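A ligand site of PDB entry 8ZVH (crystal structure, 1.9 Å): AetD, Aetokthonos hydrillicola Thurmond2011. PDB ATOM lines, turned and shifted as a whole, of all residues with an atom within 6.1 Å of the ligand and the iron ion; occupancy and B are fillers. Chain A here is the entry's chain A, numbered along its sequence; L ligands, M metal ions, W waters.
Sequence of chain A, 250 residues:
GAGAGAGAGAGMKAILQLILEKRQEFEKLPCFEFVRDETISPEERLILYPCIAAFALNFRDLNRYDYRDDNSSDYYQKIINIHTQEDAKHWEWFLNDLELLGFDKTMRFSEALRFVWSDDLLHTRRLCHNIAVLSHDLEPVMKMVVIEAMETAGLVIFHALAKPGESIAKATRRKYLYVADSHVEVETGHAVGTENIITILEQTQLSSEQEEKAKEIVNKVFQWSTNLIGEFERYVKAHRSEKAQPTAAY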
ATOM      1  N   ILE A  52      19.789  -8.092  14.152  1.00  0.00           N
ATOM      2  CA  ILE A  52      19.743  -8.005  12.654  1.00  0.00           C
ATOM      3  C   ILE A  52      20.607  -9.146  12.067  1.00  0.00           C
ATOM      4  O   ILE A  52      20.358  -9.525  10.895  1.00  0.00           O
ATOM      5  CB  ILE A  52      20.150  -6.603  12.161  1.00  0.00           C
ATOM      6  CG1 ILE A  52      19.225  -5.512  12.703  1.00  0.00           C
ATOM      7  CG2 ILE A  52      20.181  -6.562  10.650  1.00  0.00           C
ATOM      8  CD1 ILE A  52      19.837  -4.129  12.608  1.00  0.00           C
ATOM      9  N   PHE A  55      19.134 -11.888  10.170  1.00  0.00           N
ATOM     10  CA  PHE A  55      18.407 -11.360   8.965  1.00  0.00           C
ATOM     11  C   PHE A  55      19.399 -10.901   7.883  1.00  0.00           C
ATOM     12  O   PHE A  55      19.177 -11.206   6.699  1.00  0.00           O
ATOM     13  CB  PHE A  55      17.458 -10.199   9.292  1.00  0.00           C
ATOM     14  CG  PHE A  55      17.002  -9.488   8.052  1.00  0.00           C
ATOM     15  CD1 PHE A  55      15.967 -10.005   7.288  1.00  0.00           C
ATOM     16  CD2 PHE A  55      17.683  -8.384   7.571  1.00  0.00           C
ATOM     17  CE1 PHE A  55      15.598  -9.425   6.084  1.00  0.00           C
ATOM     18  CE2 PHE A  55      17.335  -7.817   6.354  1.00  0.00           C
ATOM     19  CZ  PHE A  55      16.309  -8.342   5.611  1.00  0.00           C
ATOM     20  N   ALA A  56      20.396 -10.116   8.257  1.00  0.00           N
ATOM     21  CA  ALA A  56      21.313  -9.438   7.305  1.00  0.00           C
ATOM     22  C   ALA A  56      21.975 -10.457   6.373  1.00  0.00           C
ATOM     23  O   ALA A  56      21.995 -10.239   5.170  1.00  0.00           O
ATOM     24  CB  ALA A  56      22.359  -8.672   8.057  1.00  0.00           C
ATOM     25  N   PHE A  59      19.576 -12.247   4.115  1.00  0.00           N
ATOM     26  CA  PHE A  59      19.164 -11.340   3.032  1.00  0.00           C
ATOM     27  C   PHE A  59      20.169 -11.412   1.859  1.00  0.00           C
ATOM     28  O   PHE A  59      19.757 -11.359   0.659  1.00  0.00           O
ATOM     29  CB  PHE A  59      19.021  -9.916   3.542  1.00  0.00           C
ATOM     30  CG  PHE A  59      18.474  -9.016   2.477  1.00  0.00           C
ATOM     31  CD1 PHE A  59      17.134  -9.064   2.141  1.00  0.00           C
ATOM     32  CD2 PHE A  59      19.306  -8.131   1.794  1.00  0.00           C
ATOM     33  CE1 PHE A  59      16.629  -8.258   1.127  1.00  0.00           C
ATOM     34  CE2 PHE A  59      18.794  -7.328   0.787  1.00  0.00           C
ATOM     35  CZ  PHE A  59      17.471  -7.402   0.443  1.00  0.00           C
ATOM     36  N   ASP A  87      22.715  -5.037  -3.756  1.00  0.00           N
ATOM     37  CA  ASP A  87      21.964  -5.148  -2.461  1.00  0.00           C
ATOM     38  C   ASP A  87      22.520  -6.307  -1.619  1.00  0.00           C
ATOM     39  O   ASP A  87      22.370  -6.276  -0.367  1.00  0.00           O
ATOM     40  CB  ASP A  87      20.488  -5.388  -2.725  1.00  0.00           C
ATOM     41  CG  ASP A  87      19.777  -4.250  -3.451  1.00  0.00           C
ATOM     42  OD1 ASP A  87      20.232  -3.108  -3.332  1.00  0.00           O
ATOM     43  OD2 ASP A  87      18.737  -4.542  -4.116  1.00  0.00           O
ATOM     44  N   HIS A  90      25.623  -5.494   1.322  1.00  0.00           N
ATOM     45  CA  HIS A  90      25.416  -4.651   2.512  1.00  0.00           C
ATOM     46  C   HIS A  90      25.744  -5.421   3.802  1.00  0.00           C
ATOM     47  O   HIS A  90      25.917  -4.804   4.841  1.00  0.00           O
ATOM     48  CB  HIS A  90      23.998  -4.081   2.522  1.00  0.00           C
ATOM     49  CG  HIS A  90      23.703  -3.240   1.320  1.00  0.00           C
ATOM     50  ND1 HIS A  90      22.436  -2.749   1.083  1.00  0.00           N
ATOM     51  CD2 HIS A  90      24.472  -2.842   0.273  1.00  0.00           C
ATOM     52  CE1 HIS A  90      22.430  -2.067  -0.042  1.00  0.00           C
ATOM     53  NE2 HIS A  90      23.657  -2.105  -0.570  1.00  0.00           N
ATOM     54  N   TRP A  91      25.845  -6.752   3.733  1.00  0.00           N
ATOM     55  CA  TRP A  91      26.085  -7.549   4.956  1.00  0.00           C
ATOM     56  C   TRP A  91      27.444  -7.205   5.563  1.00  0.00           C
ATOM     57  O   TRP A  91      27.571  -7.244   6.779  1.00  0.00           O
ATOM     58  CB  TRP A  91      25.929  -9.018   4.642  1.00  0.00           C
ATOM     59  CG  TRP A  91      26.953  -9.480   3.653  1.00  0.00           C
ATOM     60  CD1 TRP A  91      26.906  -9.350   2.302  1.00  0.00           C
ATOM     61  CD2 TRP A  91      28.140 -10.217   3.954  1.00  0.00           C
ATOM     62  NE1 TRP A  91      28.003  -9.931   1.735  1.00  0.00           N
ATOM     63  CE2 TRP A  91      28.791 -10.464   2.724  1.00  0.00           C
ATOM     64  CE3 TRP A  91      28.736 -10.661   5.129  1.00  0.00           C
ATOM     65  CZ2 TRP A  91      29.997 -11.157   2.638  1.00  0.00           C
ATOM     66  CZ3 TRP A  91      29.948 -11.331   5.046  1.00  0.00           C
ATOM     67  CH2 TRP A  91      30.570 -11.556   3.809  1.00  0.00           C
ATOM     68  N   TRP A  93      28.627  -4.213   5.590  1.00  0.00           N
ATOM     69  CA  TRP A  93      28.332  -2.953   6.307  1.00  0.00           C
ATOM     70  C   TRP A  93      27.751  -3.340   7.682  1.00  0.00           C
ATOM     71  O   TRP A  93      28.175  -2.758   8.672  1.00  0.00           O
ATOM     72  CB  TRP A  93      27.408  -2.046   5.515  1.00  0.00           C
ATOM     73  CG  TRP A  93      27.907  -1.648   4.165  1.00  0.00           C
ATOM     74  CD1 TRP A  93      29.179  -1.756   3.655  1.00  0.00           C
ATOM     75  CD2 TRP A  93      27.108  -1.051   3.131  1.00  0.00           C
ATOM     76  NE1 TRP A  93      29.216  -1.261   2.380  1.00  0.00           N
ATOM     77  CE2 TRP A  93      27.967  -0.809   2.034  1.00  0.00           C
ATOM     78  CE3 TRP A  93      25.773  -0.647   3.045  1.00  0.00           C
ATOM     79  CZ2 TRP A  93      27.496  -0.245   0.850  1.00  0.00           C
ATOM     80  CZ3 TRP A  93      25.328  -0.055   1.887  1.00  0.00           C
ATOM     81  CH2 TRP A  93      26.175   0.109   0.789  1.00  0.00           C
ATOM     82  N   PHE A  94      26.847  -4.323   7.730  1.00  0.00           N
ATOM     83  CA  PHE A  94      26.273  -4.827   8.994  1.00  0.00           C
ATOM     84  C   PHE A  94      27.412  -5.192   9.967  1.00  0.00           C
ATOM     85  O   PHE A  94      27.410  -4.828  11.148  1.00  0.00           O
ATOM     86  CB  PHE A  94      25.318  -5.990   8.759  1.00  0.00           C
ATOM     87  CG  PHE A  94      24.996  -6.703  10.035  1.00  0.00           C
ATOM     88  CD1 PHE A  94      24.130  -6.139  10.966  1.00  0.00           C
ATOM     89  CD2 PHE A  94      25.637  -7.892  10.374  1.00  0.00           C
ATOM     90  CE1 PHE A  94      23.905  -6.730  12.205  1.00  0.00           C
ATOM     91  CE2 PHE A  94      25.393  -8.489  11.603  1.00  0.00           C
ATOM     92  CZ  PHE A  94      24.543  -7.918  12.508  1.00  0.00           C
ATOM     93  N   LEU A 127      12.331 -14.577   7.840  1.00  0.00           N
ATOM     94  CA  LEU A 127      11.775 -13.610   6.845  1.00  0.00           C
ATOM     95  C   LEU A 127      12.260 -13.945   5.416  1.00  0.00           C
ATOM     96  O   LEU A 127      11.404 -14.154   4.509  1.00  0.00           O
ATOM     97  CB  LEU A 127      12.119 -12.165   7.248  1.00  0.00           C
ATOM     98  CG  LEU A 127      11.674 -11.134   6.203  1.00  0.00           C
ATOM     99  CD1 LEU A 127      10.177 -11.171   5.964  1.00  0.00           C
ATOM    100  CD2 LEU A 127      12.086  -9.742   6.628  1.00  0.00           C
ATOM    101  N   MET A 150       9.222  -5.511  -0.340  1.00  0.00           N
ATOM    102  CA  MET A 150      10.269  -5.816   0.667  1.00  0.00           C
ATOM    103  C   MET A 150      11.110  -4.553   0.869  1.00  0.00           C
ATOM    104  O   MET A 150      11.376  -4.178   2.041  1.00  0.00           O
ATOM    105  CB  MET A 150      11.192  -6.930   0.144  1.00  0.00           C
ATOM    106  CG  MET A 150      10.991  -8.238   0.803  1.00  0.00           C
ATOM    107  SD  MET A 150      11.539  -8.139   2.497  1.00  0.00           S
ATOM    108  CE  MET A 150      13.217  -8.733   2.312  1.00  0.00           C
ATOM    109  N   GLU A 151      11.546  -3.960  -0.240  1.00  0.00           N
ATOM    110  CA  GLU A 151      12.443  -2.781  -0.221  1.00  0.00           C
ATOM    111  C   GLU A 151      11.711  -1.595   0.395  1.00  0.00           C
ATOM    112  O   GLU A 151      12.372  -0.772   1.118  1.00  0.00           O
ATOM    113  CB  GLU A 151      12.970  -2.507  -1.631  1.00  0.00           C
ATOM    114  CG  GLU A 151      14.157  -3.391  -1.986  1.00  0.00           C
ATOM    115  CD  GLU A 151      15.412  -3.021  -1.198  1.00  0.00           C
ATOM    116  OE1 GLU A 151      15.375  -2.081  -0.371  1.00  0.00           O
ATOM    117  OE2 GLU A 151      16.415  -3.628  -1.426  1.00  0.00           O
ATOM    118  N   THR A 152      10.399  -1.504   0.188  1.00  0.00           N
ATOM    119  CA  THR A 152       9.564  -0.427   0.778  1.00  0.00           C
ATOM    120  C   THR A 152       9.679  -0.524   2.301  1.00  0.00           C
ATOM    121  O   THR A 152       9.976   0.496   2.911  1.00  0.00           O
ATOM    122  CB  THR A 152       8.116  -0.460   0.280  1.00  0.00           C
ATOM    123  OG1 THR A 152       8.114  -0.267  -1.133  1.00  0.00           O
ATOM    124  CG2 THR A 152       7.249   0.579   0.943  1.00  0.00           C
ATOM    125  N   ALA A 153       9.525  -1.724   2.874  1.00  0.00           N
ATOM    126  CA  ALA A 153       9.719  -1.999   4.308  1.00  0.00           C
ATOM    127  C   ALA A 153      11.164  -1.717   4.730  1.00  0.00           C
ATOM    128  O   ALA A 153      11.358  -1.106   5.806  1.00  0.00           O
ATOM    129  CB  ALA A 153       9.298  -3.414   4.621  1.00  0.00           C
ATOM    130  N   GLY A 154      12.164  -2.204   3.987  1.00  0.00           N
ATOM    131  CA  GLY A 154      13.584  -1.945   4.291  1.00  0.00           C
ATOM    132  C   GLY A 154      13.862  -0.452   4.438  1.00  0.00           C
ATOM    133  O   GLY A 154      14.598  -0.023   5.393  1.00  0.00           O
ATOM    134  N   LEU A 155      13.351   0.345   3.509  1.00  0.00           N
ATOM    135  CA  LEU A 155      13.645   1.802   3.483  1.00  0.00           C
ATOM    136  C   LEU A 155      13.030   2.432   4.744  1.00  0.00           C
ATOM    137  O   LEU A 155      13.680   3.301   5.350  1.00  0.00           O
ATOM    138  CB  LEU A 155      13.111   2.445   2.202  1.00  0.00           C
ATOM    139  CG  LEU A 155      13.796   2.012   0.907  1.00  0.00           C
ATOM    140  CD1 LEU A 155      13.351   2.901  -0.237  1.00  0.00           C
ATOM    141  CD2 LEU A 155      15.326   2.025   1.047  1.00  0.00           C
ATOM    142  N   ILE A 157      12.679   0.807   7.677  1.00  0.00           N
ATOM    143  CA  ILE A 157      13.516   0.272   8.783  1.00  0.00           C
ATOM    144  C   ILE A 157      14.793   1.112   8.883  1.00  0.00           C
ATOM    145  O   ILE A 157      15.168   1.520   9.988  1.00  0.00           O
ATOM    146  CB  ILE A 157      13.848  -1.222   8.566  1.00  0.00           C
ATOM    147  CG1 ILE A 157      12.626  -2.137   8.762  1.00  0.00           C
ATOM    148  CG2 ILE A 157      14.983  -1.584   9.488  1.00  0.00           C
ATOM    149  CD1 ILE A 157      12.838  -3.554   8.208  1.00  0.00           C
ATOM    150  N   PHE A 158      15.502   1.249   7.772  1.00  0.00           N
ATOM    151  CA  PHE A 158      16.838   1.854   7.733  1.00  0.00           C
ATOM    152  C   PHE A 158      16.751   3.368   7.841  1.00  0.00           C
ATOM    153  O   PHE A 158      17.641   3.962   8.431  1.00  0.00           O
ATOM    154  CB  PHE A 158      17.612   1.308   6.533  1.00  0.00           C
ATOM    155  CG  PHE A 158      18.096  -0.074   6.857  1.00  0.00           C
ATOM    156  CD1 PHE A 158      19.170  -0.242   7.723  1.00  0.00           C
ATOM    157  CD2 PHE A 158      17.369  -1.178   6.479  1.00  0.00           C
ATOM    158  CE1 PHE A 158      19.562  -1.513   8.122  1.00  0.00           C
ATOM    159  CE2 PHE A 158      17.767  -2.447   6.886  1.00  0.00           C
ATOM    160  CZ  PHE A 158      18.869  -2.612   7.690  1.00  0.00           C
ATOM    161  N   TYR A 178      25.980   0.844   7.759  1.00  0.00           N
ATOM    162  CA  TYR A 178      24.734   0.041   7.743  1.00  0.00           C
ATOM    163  C   TYR A 178      23.560   0.817   8.330  1.00  0.00           C
ATOM    164  O   TYR A 178      22.530   0.935   7.648  1.00  0.00           O
ATOM    165  CB  TYR A 178      24.978  -1.304   8.445  1.00  0.00           C
ATOM    166  CG  TYR A 178      23.912  -2.347   8.220  1.00  0.00           C
ATOM    167  CD1 TYR A 178      23.768  -2.973   7.003  1.00  0.00           C
ATOM    168  CD2 TYR A 178      23.041  -2.706   9.248  1.00  0.00           C
ATOM    169  CE1 TYR A 178      22.790  -3.922   6.779  1.00  0.00           C
ATOM    170  CE2 TYR A 178      22.077  -3.684   9.058  1.00  0.00           C
ATOM    171  CZ  TYR A 178      21.932  -4.276   7.809  1.00  0.00           C
ATOM    172  OH  TYR A 178      20.978  -5.226   7.580  1.00  0.00           O
ATOM    173  N   HIS A 183      23.408   4.096   3.346  1.00  0.00           N
ATOM    174  CA  HIS A 183      22.746   2.796   3.062  1.00  0.00           C
ATOM    175  C   HIS A 183      21.378   3.045   2.439  1.00  0.00           C
ATOM    176  O   HIS A 183      21.089   2.441   1.385  1.00  0.00           O
ATOM    177  CB  HIS A 183      22.690   1.965   4.346  1.00  0.00           C
ATOM    178  CG  HIS A 183      22.143   0.593   4.141  1.00  0.00           C
ATOM    179  ND1 HIS A 183      21.866  -0.227   5.197  1.00  0.00           N
ATOM    180  CD2 HIS A 183      21.773  -0.089   3.039  1.00  0.00           C
ATOM    181  CE1 HIS A 183      21.386  -1.377   4.762  1.00  0.00           C
ATOM    182  NE2 HIS A 183      21.319  -1.332   3.458  1.00  0.00           N
ATOM    183  N   GLU A 187      20.548   2.154  -1.543  1.00  0.00           N
ATOM    184  CA  GLU A 187      19.447   1.140  -1.604  1.00  0.00           C
ATOM    185  C   GLU A 187      18.263   1.661  -2.444  1.00  0.00           C
ATOM    186  O   GLU A 187      17.778   0.888  -3.293  1.00  0.00           O
ATOM    187  CB  GLU A 187      18.974   0.779  -0.191  1.00  0.00           C
ATOM    188  CG  GLU A 187      18.080  -0.458  -0.123  1.00  0.00           C
ATOM    189  CD  GLU A 187      18.789  -1.726   0.334  1.00  0.00           C
ATOM    190  OE1 GLU A 187      19.758  -1.584   1.101  1.00  0.00           O
ATOM    191  OE2 GLU A 187      18.376  -2.854  -0.094  1.00  0.00           O
ATOM    192  N   SER A 225       7.386  -8.723   7.755  1.00  0.00           N
ATOM    193  CA  SER A 225       8.200  -7.559   8.180  1.00  0.00           C
ATOM    194  C   SER A 225       7.748  -7.081   9.553  1.00  0.00           C
ATOM    195  O   SER A 225       8.610  -6.898  10.408  1.00  0.00           O
ATOM    196  CB  SER A 225       8.173  -6.476   7.141  1.00  0.00           C
ATOM    197  OG  SER A 225       8.717  -6.953   5.903  1.00  0.00           O
HETATM  198  N1  LIG L   1      18.911  -3.192   3.387  1.00  0.00           N
HETATM  199  C1  LIG L   1      18.961  -4.443   4.198  1.00  0.00           C
HETATM  200  C2  LIG L   1      20.421  -4.910   4.301  1.00  0.00           C
HETATM  201  O1  LIG L   1      20.681  -5.879   5.040  1.00  0.00           O
HETATM  202  C3  LIG L   1      18.092  -5.536   3.555  1.00  0.00           C
HETATM  203  C4  LIG L   1      16.600  -5.371   3.670  1.00  0.00           C
HETATM  204  C5  LIG L   1      15.979  -5.273   4.895  1.00  0.00           C
HETATM  205  C6  LIG L   1      15.820  -5.293   2.525  1.00  0.00           C
HETATM  206  C7  LIG L   1      14.599  -5.164   4.999  1.00  0.00           C
HETATM  207  C8  LIG L   1      14.444  -5.171   2.623  1.00  0.00           C
HETATM  208  C9  LIG L   1      13.842  -5.108   3.853  1.00  0.00           C
HETATM  209  O2  LIG L   1      21.400  -4.360   3.690  1.00  0.00           O
HETATM  210 FE    FE M   1      20.643  -2.952   2.359  1.00  0.00          FE
HETATM  211  O   HOH W   1      22.482  -7.557   4.262  1.00  0.00           O
HETATM  212  O   HOH W   2      20.112  -4.344   0.993  1.00  0.00           O
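The side-chain hydroxyl of Tyr 178 lies within hydrogen-bond range of an oxygen (O1) of the ligand (2.6 Å).
OE2 of Glu 151 lies close to OE2 of Glu 187 (2.5 Å).
A ring nitrogen (ND1) of His 183 sits at hydrogen-bond distance from the backbone carbonyl oxygen (O) of Tyr 178, at 2.8 Å.
Merely in contact with the ligand: Phe 55 (3.2 Å), Met 150 (3.2 Å), Gly 154 (3.2 Å), Phe 59 (3.4 Å), Phe 158 (3.6 Å) and Ile 157 (3.999 Å).
Hydrophobic or aromatic side chains that line the ligand: Phe 55, Phe 59, His 90, Met 150, Ile 157, Phe 158, Tyr 178 and His 183.
Along chain A the residues within 4 Å of the ligand span positions 55 to 187.
Of the 22 residues printed, 3 come within 4 Å of the iron ion.
The nearest printed residue that does not touch the iron ion is Asp 87 (4.6 Å).
The iron ion is bound by water W2, a nitrogen (N1) of the ligand, the side-chain carboxylate of Glu 187, a ring nitrogen (NE2) of His 183, an oxygen (O2) of the ligand and a ring nitrogen (ND1) of His 90.
The iron ion has six donor atoms within binding distance.
Water W2 lies within hydrogen-bond range of the side-chain carboxylate of Glu 187 (2.5 Å) and the backbone carbonyl oxygen of Asp 87 (3.3 Å).
Water W1 lies within hydrogen-bond range of O1 of the ligand, O of Ala 56 and N of Trp 91.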
